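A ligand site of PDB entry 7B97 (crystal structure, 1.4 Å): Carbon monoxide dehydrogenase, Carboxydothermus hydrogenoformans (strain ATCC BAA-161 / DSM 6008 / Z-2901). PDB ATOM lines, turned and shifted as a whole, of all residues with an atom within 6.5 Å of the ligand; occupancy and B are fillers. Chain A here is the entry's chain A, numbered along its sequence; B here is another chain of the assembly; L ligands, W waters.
Water W1 lies within hydrogen-bond range of the side-chain amide nitrogen of Asn 52, a sulfur (S4) of the ligand and the side-chain sulfur of Met 555 of chain B.
SG of Cys 50 sits close to SD of Met 555 of chain B (3.6 Å).
The backbone NH (N) of Cys 47 sits at hydrogen-bond distance from the backbone carbonyl oxygen (O) of Cys 55 (2.8 Å).
The side-chain sulfur (SG) of Cys 47 sits close to the guanidinium group (NH2) of Arg 78 (3.4 Å).
The side-chain sulfur of Cys 68 lies close to the backbone NH of Ile 70, 3.6 Å away.
O of Arg 78 is in hydrogen-bond range of SG of Cys 194.
NH2 of Arg 37 of chain B lies close to O of Gly 53 (3.5 Å).
The side-chain sulfur (SD) of Met 75 sits close to the backbone NH (N) of Ser 46 (3.6 Å).
NH2 of Arg 37 of chain B sits at hydrogen-bond distance from O of Asn 52.
The backbone NH of Cys 50 sits close to a sulfur (S3) of the ligand.
The side-chain sulfur (SG) of Cys 50 is bound to an iron atom (FE2) of the ligand.
The side-chain sulfur of Cys 55 binds an iron atom (FE1) of the ligand (2.3 Å).
The side-chain sulfur of Cys 47 is bound to an iron atom (FE4) of the ligand.
The backbone NH of Cys 68 lies close to a sulfur (S4) of the ligand.
FE3 of the ligand is bound by SG of Cys 68 (2.3 Å).
A sulfur (S1) of the ligand lies close to the side-chain hydroxyl of Thr 196.
The guanidinium group (NH2) of Arg 78 lies close to a sulfur (S1) of the ligand, 3.4 Å away.
N of Gly 53 sits close to S3 of the ligand.
S4 of the ligand lies close to N of Val 67, at 3.7 Å.
A sulfur (S3) of the ligand lies close to the backbone NH (N) of Leu 49 (3.8 Å).
Asn 52 touches the ligand (CB to S4, 3.8 Å).
Gly 66 touches the ligand.
CG2 of Ile 70 touches S2 of the ligand (3.7 Å).
Met 75 touches the ligand (CE to S2, 3.7 Å).
Hydrophobic or aromatic side chains within 4 Å of the ligand: Val 67, Ile 70 and Met 75.
Along chain A the residues within 4 Å of the ligand span positions 47 to 196.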
ATOM      1  N   SER A  46      15.330   2.831 -11.214  1.00  0.00           N
ATOM      2  CA  SER A  46      14.501   1.639 -11.152  1.00  0.00           C
ATOM      3  C   SER A  46      13.791   1.615  -9.803  1.00  0.00           C
ATOM      4  O   SER A  46      14.213   2.262  -8.840  1.00  0.00           O
ATOM      5  CB  SER A  46      15.371   0.379 -11.280  1.00  0.00           C
ATOM      6  OG  SER A  46      16.162   0.199 -10.116  1.00  0.00           O
ATOM      7  N   CYS A  47      12.741   0.807  -9.730  1.00  0.00           N
ATOM      8  CA  CYS A  47      11.954   0.725  -8.508  1.00  0.00           C
ATOM      9  C   CYS A  47      11.342  -0.663  -8.401  1.00  0.00           C
ATOM     10  O   CYS A  47      10.806  -1.192  -9.362  1.00  0.00           O
ATOM     11  CB  CYS A  47      10.853   1.776  -8.480  1.00  0.00           C
ATOM     12  SG  CYS A  47       9.967   1.854  -6.881  1.00  0.00           S
ATOM     13  N   GLN A  48      11.426  -1.235  -7.200  1.00  0.00           N
ATOM     14  CA  GLN A  48      10.872  -2.553  -6.917  1.00  0.00           C
ATOM     15  C   GLN A  48       9.926  -2.536  -5.712  1.00  0.00           C
ATOM     16  O   GLN A  48       9.747  -3.558  -5.043  1.00  0.00           O
ATOM     17  CB  GLN A  48      11.978  -3.578  -6.705  1.00  0.00           C
ATOM     18  CG  GLN A  48      13.036  -3.654  -7.771  1.00  0.00           C
ATOM     19  CD  GLN A  48      14.051  -2.543  -7.699  1.00  0.00           C
ATOM     20  OE1 GLN A  48      14.382  -2.037  -6.614  1.00  0.00           O
ATOM     21  NE2 GLN A  48      14.554  -2.140  -8.852  1.00  0.00           N
ATOM     22  N   LEU A  49       9.316  -1.401  -5.418  1.00  0.00           N
ATOM     23  CA  LEU A  49       8.624  -1.285  -4.151  1.00  0.00           C
ATOM     24  C   LEU A  49       7.192  -1.790  -4.161  1.00  0.00           C
ATOM     25  O   LEU A  49       6.614  -1.955  -3.087  1.00  0.00           O
ATOM     26  CB  LEU A  49       8.681   0.163  -3.631  1.00  0.00           C
ATOM     27  CG  LEU A  49      10.102   0.670  -3.327  1.00  0.00           C
ATOM     28  CD1 LEU A  49       9.960   2.046  -2.679  1.00  0.00           C
ATOM     29  CD2 LEU A  49      10.932  -0.290  -2.493  1.00  0.00           C
ATOM     30  N   CYS A  50       6.606  -2.096  -5.317  1.00  0.00           N
ATOM     31  CA  CYS A  50       5.259  -2.658  -5.298  1.00  0.00           C
ATOM     32  C   CYS A  50       5.055  -3.575  -6.494  1.00  0.00           C
ATOM     33  O   CYS A  50       5.898  -3.684  -7.398  1.00  0.00           O
ATOM     34  CB  CYS A  50       4.187  -1.562  -5.261  1.00  0.00           C
ATOM     35  SG  CYS A  50       3.721  -0.881  -6.876  1.00  0.00           S
ATOM     36  N   SER A  51       3.911  -4.239  -6.490  1.00  0.00           N
ATOM     37  CA  SER A  51       3.692  -5.294  -7.466  1.00  0.00           C
ATOM     38  C   SER A  51       3.467  -4.769  -8.881  1.00  0.00           C
ATOM     39  O   SER A  51       3.532  -5.572  -9.821  1.00  0.00           O
ATOM     40  CB  SER A  51       2.508  -6.189  -7.092  1.00  0.00           C
ATOM     41  OG  SER A  51       1.266  -5.532  -7.290  1.00  0.00           O
ATOM     42  N   ASN A  52       3.130  -3.492  -9.060  1.00  0.00           N
ATOM     43  CA  ASN A  52       3.041  -2.936 -10.414  1.00  0.00           C
ATOM     44  C   ASN A  52       4.406  -2.788 -11.071  1.00  0.00           C
ATOM     45  O   ASN A  52       4.482  -2.585 -12.274  1.00  0.00           O
ATOM     46  CB  ASN A  52       2.333  -1.571 -10.426  1.00  0.00           C
ATOM     47  CG  ASN A  52       0.827  -1.673 -10.367  1.00  0.00           C
ATOM     48  OD1 ASN A  52       0.213  -2.453 -11.073  1.00  0.00           O
ATOM     49  ND2 ASN A  52       0.222  -0.858  -9.511  1.00  0.00           N
ATOM     50  N   GLY A  53       5.476  -2.864 -10.289  1.00  0.00           N
ATOM     51  CA  GLY A  53       6.806  -2.894 -10.824  1.00  0.00           C
ATOM     52  C   GLY A  53       7.196  -4.276 -11.308  1.00  0.00           C
ATOM     53  O   GLY A  53       6.345  -5.154 -11.504  1.00  0.00           O
ATOM     54  N   PRO A  54       8.502  -4.505 -11.519  1.00  0.00           N
ATOM     55  CA  PRO A  54       9.552  -3.501 -11.348  1.00  0.00           C
ATOM     56  C   PRO A  54       9.440  -2.377 -12.395  1.00  0.00           C
ATOM     57  O   PRO A  54       9.088  -2.654 -13.558  1.00  0.00           O
ATOM     58  CB  PRO A  54      10.840  -4.303 -11.521  1.00  0.00           C
ATOM     59  CG  PRO A  54      10.451  -5.425 -12.419  1.00  0.00           C
ATOM     60  CD  PRO A  54       9.019  -5.766 -12.069  1.00  0.00           C
ATOM     61  N   CYS A  55       9.659  -1.151 -11.977  1.00  0.00           N
ATOM     62  CA  CYS A  55       9.531  -0.005 -12.874  1.00  0.00           C
ATOM     63  C   CYS A  55      10.909   0.564 -13.185  1.00  0.00           C
ATOM     64  O   CYS A  55      11.841   0.439 -12.391  1.00  0.00           O
ATOM     65  CB  CYS A  55       8.678   1.094 -12.243  1.00  0.00           C
ATOM     66  SG  CYS A  55       6.925   0.686 -12.171  1.00  0.00           S
ATOM     67  N   ARG A  56      10.986   1.254 -14.315  1.00  0.00           N
ATOM     68  CA  ARG A  56      12.191   1.901 -14.829  1.00  0.00           C
ATOM     69  C   ARG A  56      11.773   3.223 -15.447  1.00  0.00           C
ATOM     70  O   ARG A  56      10.693   3.320 -16.051  1.00  0.00           O
ATOM     71  CB  ARG A  56      12.885   1.068 -15.919  1.00  0.00           C
ATOM     72  CG  ARG A  56      13.599  -0.133 -15.351  1.00  0.00           C
ATOM     73  CD  ARG A  56      13.944  -1.112 -16.444  1.00  0.00           C
ATOM     74  NE  ARG A  56      15.045  -1.946 -16.010  1.00  0.00           N
ATOM     75  CZ  ARG A  56      15.725  -2.779 -16.776  1.00  0.00           C
ATOM     76  NH1 ARG A  56      15.360  -2.948 -18.029  1.00  0.00           N
ATOM     77  NH2 ARG A  56      16.763  -3.430 -16.272  1.00  0.00           N
ATOM     78  N   ILE A  57      12.610   4.237 -15.295  1.00  0.00           N
ATOM     79  CA  ILE A  57      12.420   5.492 -16.022  1.00  0.00           C
ATOM     80  C   ILE A  57      13.292   5.477 -17.273  1.00  0.00           C
ATOM     81  O   ILE A  57      14.522   5.378 -17.194  1.00  0.00           O
ATOM     82  CB  ILE A  57      12.765   6.711 -15.140  1.00  0.00           C
ATOM     83  CG1 ILE A  57      11.973   6.702 -13.821  1.00  0.00           C
ATOM     84  CG2 ILE A  57      12.510   7.991 -15.952  1.00  0.00           C
ATOM     85  CD1 ILE A  57      10.463   6.650 -13.964  1.00  0.00           C
ATOM     86  N   LEU A  65       7.225   8.060 -16.037  1.00  0.00           N
ATOM     87  CA  LEU A  65       6.862   7.902 -14.637  1.00  0.00           C
ATOM     88  C   LEU A  65       6.675   6.425 -14.353  1.00  0.00           C
ATOM     89  O   LEU A  65       6.391   5.610 -15.243  1.00  0.00           O
ATOM     90  CB  LEU A  65       5.545   8.604 -14.364  1.00  0.00           C
ATOM     91  CG  LEU A  65       5.532  10.113 -14.649  1.00  0.00           C
ATOM     92  CD1 LEU A  65       4.123  10.669 -14.472  1.00  0.00           C
ATOM     93  CD2 LEU A  65       6.503  10.920 -13.784  1.00  0.00           C
ATOM     94  N   GLY A  66       6.830   6.055 -13.079  1.00  0.00           N
ATOM     95  CA  GLY A  66       6.427   4.730 -12.644  1.00  0.00           C
ATOM     96  C   GLY A  66       4.932   4.552 -12.778  1.00  0.00           C
ATOM     97  O   GLY A  66       4.175   5.487 -12.997  1.00  0.00           O
ATOM     98  N   VAL A  67       4.478   3.291 -12.650  1.00  0.00           N
ATOM     99  CA  VAL A  67       3.057   3.029 -12.855  1.00  0.00           C
ATOM    100  C   VAL A  67       2.216   3.905 -11.924  1.00  0.00           C
ATOM    101  O   VAL A  67       1.184   4.460 -12.322  1.00  0.00           O
ATOM    102  CB  VAL A  67       2.726   1.544 -12.695  1.00  0.00           C
ATOM    103  CG1 VAL A  67       1.222   1.363 -12.783  1.00  0.00           C
ATOM    104  CG2 VAL A  67       3.420   0.732 -13.777  1.00  0.00           C
ATOM    105  N   CYS A  68       2.676   4.047 -10.674  1.00  0.00           N
ATOM    106  CA  CYS A  68       1.948   4.824  -9.664  1.00  0.00           C
ATOM    107  C   CYS A  68       1.947   6.326  -9.945  1.00  0.00           C
ATOM    108  O   CYS A  68       1.172   7.063  -9.310  1.00  0.00           O
ATOM    109  CB  CYS A  68       2.590   4.593  -8.290  1.00  0.00           C
ATOM    110  SG  CYS A  68       4.315   5.066  -8.237  1.00  0.00           S
ATOM    111  N   GLY A  69       2.823   6.801 -10.818  1.00  0.00           N
ATOM    112  CA  GLY A  69       2.951   8.211 -11.154  1.00  0.00           C
ATOM    113  C   GLY A  69       4.200   8.892 -10.600  1.00  0.00           C
ATOM    114  O   GLY A  69       4.395  10.076 -10.841  1.00  0.00           O
ATOM    115  N   ILE A  70       5.075   8.190  -9.897  1.00  0.00           N
ATOM    116  CA  ILE A  70       6.255   8.856  -9.333  1.00  0.00           C
ATOM    117  C   ILE A  70       7.256   9.160 -10.437  1.00  0.00           C
ATOM    118  O   ILE A  70       7.427   8.388 -11.396  1.00  0.00           O
ATOM    119  CB  ILE A  70       6.846   8.013  -8.197  1.00  0.00           C
ATOM    120  CG1 ILE A  70       7.723   8.887  -7.271  1.00  0.00           C
ATOM    121  CG2 ILE A  70       7.644   6.811  -8.721  1.00  0.00           C
ATOM    122  CD1 ILE A  70       8.253   8.141  -6.053  1.00  0.00           C
ATOM    123  N   MET A  75      11.573   8.760  -7.195  1.00  0.00           N
ATOM    124  CA  MET A  75      12.004   7.376  -7.136  1.00  0.00           C
ATOM    125  C   MET A  75      13.382   7.241  -6.511  1.00  0.00           C
ATOM    126  O   MET A  75      13.604   6.430  -5.603  1.00  0.00           O
ATOM    127  CB  MET A  75      12.008   6.799  -8.567  1.00  0.00           C
ATOM    128  CG  MET A  75      12.388   5.338  -8.664  1.00  0.00           C
ATOM    129  SD  MET A  75      12.349   4.771 -10.434  1.00  0.00           S
ATOM    130  CE  MET A  75      10.594   4.838 -10.726  1.00  0.00           C
ATOM    131  N   ARG A  78      13.544   8.374  -2.758  1.00  0.00           N
ATOM    132  CA  ARG A  78      12.788   7.470  -1.907  1.00  0.00           C
ATOM    133  C   ARG A  78      13.596   6.230  -1.567  1.00  0.00           C
ATOM    134  O   ARG A  78      13.582   5.765  -0.428  1.00  0.00           O
ATOM    135  CB  ARG A  78      11.460   7.107  -2.574  1.00  0.00           C
ATOM    136  CG  ARG A  78      10.619   6.188  -1.696  1.00  0.00           C
ATOM    137  CD  ARG A  78       9.228   5.964  -2.265  1.00  0.00           C
ATOM    138  NE  ARG A  78       9.316   5.406  -3.600  1.00  0.00           N
ATOM    139  CZ  ARG A  78       8.245   5.110  -4.330  1.00  0.00           C
ATOM    140  NH1 ARG A  78       7.023   5.338  -3.862  1.00  0.00           N
ATOM    141  NH2 ARG A  78       8.401   4.568  -5.551  1.00  0.00           N
ATOM    142  N   CYS A 194       8.077   5.904   2.648  1.00  0.00           N
ATOM    143  CA  CYS A 194       8.590   5.265   1.453  1.00  0.00           C
ATOM    144  C   CYS A 194       7.637   4.220   0.900  1.00  0.00           C
ATOM    145  O   CYS A 194       7.846   3.772  -0.238  1.00  0.00           O
ATOM    146  CB  CYS A 194       9.948   4.622   1.746  1.00  0.00           C
ATOM    147  SG  CYS A 194      11.323   5.762   2.116  1.00  0.00           S
ATOM    148  N   LEU A 195       6.605   3.836   1.638  1.00  0.00           N
ATOM    149  CA  LEU A 195       5.615   2.924   1.075  1.00  0.00           C
ATOM    150  C   LEU A 195       4.989   3.555  -0.158  1.00  0.00           C
ATOM    151  O   LEU A 195       4.826   4.780  -0.243  1.00  0.00           O
ATOM    152  CB  LEU A 195       4.533   2.623   2.104  1.00  0.00           C
ATOM    153  CG  LEU A 195       3.647   1.443   1.729  1.00  0.00           C
ATOM    154  CD1 LEU A 195       4.056   0.179   2.459  1.00  0.00           C
ATOM    155  CD2 LEU A 195       2.225   1.765   2.051  1.00  0.00           C
ATOM    156  N   THR A 196       4.647   2.716  -1.129  1.00  0.00           N
ATOM    157  CA  THR A 196       4.036   3.200  -2.361  1.00  0.00           C
ATOM    158  C   THR A 196       2.854   4.112  -2.045  1.00  0.00           C
ATOM    159  O   THR A 196       2.061   3.841  -1.131  1.00  0.00           O
ATOM    160  CB  THR A 196       3.577   2.004  -3.193  1.00  0.00           C
ATOM    161  OG1 THR A 196       4.716   1.164  -3.446  1.00  0.00           O
ATOM    162  CG2 THR A 196       2.941   2.432  -4.507  1.00  0.00           C
ATOM    163  N   ASN A 197       2.780   5.213  -2.781  1.00  0.00           N
ATOM    164  CA  ASN A 197       1.655   6.134  -2.734  1.00  0.00           C
ATOM    165  C   ASN A 197       1.545   6.853  -1.383  1.00  0.00           C
ATOM    166  O   ASN A 197       0.435   7.206  -0.956  1.00  0.00           O
ATOM    167  CB  ASN A 197       0.335   5.469  -3.110  1.00  0.00           C
ATOM    168  CG  ASN A 197       0.297   5.053  -4.564  1.00  0.00           C
ATOM    169  OD1 ASN A 197       0.955   5.664  -5.425  1.00  0.00           O
ATOM    170  ND2 ASN A 197      -0.505   4.033  -4.870  1.00  0.00           N
ATOM    171  N   GLN B  33       6.090   0.540 -19.304  1.00  0.00           N
ATOM    172  CA  GLN B  33       6.905  -0.295 -18.434  1.00  0.00           C
ATOM    173  C   GLN B  33       7.069  -1.686 -19.001  1.00  0.00           C
ATOM    174  O   GLN B  33       8.112  -2.325 -18.804  1.00  0.00           O
ATOM    175  CB  GLN B  33       6.282  -0.362 -17.042  1.00  0.00           C
ATOM    176  CG  GLN B  33       6.305   0.945 -16.254  1.00  0.00           C
ATOM    177  CD  GLN B  33       7.712   1.437 -15.976  1.00  0.00           C
ATOM    178  OE1 GLN B  33       8.622   0.624 -15.800  1.00  0.00           O
ATOM    179  NE2 GLN B  33       7.901   2.753 -15.936  1.00  0.00           N
ATOM    180  N   ARG B  37      10.692  -4.444 -19.014  1.00  0.00           N
ATOM    181  CA  ARG B  37      10.668  -5.031 -17.670  1.00  0.00           C
ATOM    182  C   ARG B  37      11.947  -5.809 -17.374  1.00  0.00           C
ATOM    183  O   ARG B  37      12.458  -6.562 -18.205  1.00  0.00           O
ATOM    184  CB  ARG B  37       9.473  -5.977 -17.483  1.00  0.00           C
ATOM    185  CG  ARG B  37       8.123  -5.315 -17.530  1.00  0.00           C
ATOM    186  CD  ARG B  37       7.827  -4.487 -16.299  1.00  0.00           C
ATOM    187  NE  ARG B  37       6.386  -4.227 -16.250  1.00  0.00           N
ATOM    188  CZ  ARG B  37       5.786  -3.559 -15.267  1.00  0.00           C
ATOM    189  NH1 ARG B  37       4.470  -3.378 -15.286  1.00  0.00           N
ATOM    190  NH2 ARG B  37       6.497  -3.065 -14.284  1.00  0.00           N
ATOM    191  N   MET B 555      -0.625  -5.366  -3.691  1.00  0.00           N
ATOM    192  CA  MET B 555       0.196  -4.297  -4.250  1.00  0.00           C
ATOM    193  C   MET B 555       1.441  -4.033  -3.418  1.00  0.00           C
ATOM    194  O   MET B 555       2.559  -4.004  -3.950  1.00  0.00           O
ATOM    195  CB  MET B 555      -0.618  -2.994  -4.383  1.00  0.00           C
ATOM    196  CG  MET B 555      -0.048  -1.959  -5.389  1.00  0.00           C
ATOM    197  SD  MET B 555       0.884  -0.582  -4.665  1.00  0.00           S
ATOM    198  CE  MET B 555      -0.438   0.393  -3.927  1.00  0.00           C
HETATM  199 FE1  LIG L   1       6.559   1.128  -9.952  1.00  0.00          FE
HETATM  200 FE2  LIG L   1       5.406   0.457  -7.600  1.00  0.00          FE
HETATM  201 FE3  LIG L   1       5.561   3.091  -8.302  1.00  0.00          FE
HETATM  202 FE4  LIG L   1       7.815   1.677  -7.661  1.00  0.00          FE
HETATM  203  S1  LIG L   1       6.085   2.192  -6.246  1.00  0.00           S
HETATM  204  S2  LIG L   1       7.528   3.147  -9.409  1.00  0.00           S
HETATM  205  S3  LIG L   1       7.328  -0.389  -8.456  1.00  0.00           S
HETATM  206  S4  LIG L   1       4.407   1.446  -9.405  1.00  0.00           S
HETATM  207  O   HOH W   1       1.270   1.093  -7.918  1.00  0.00           O
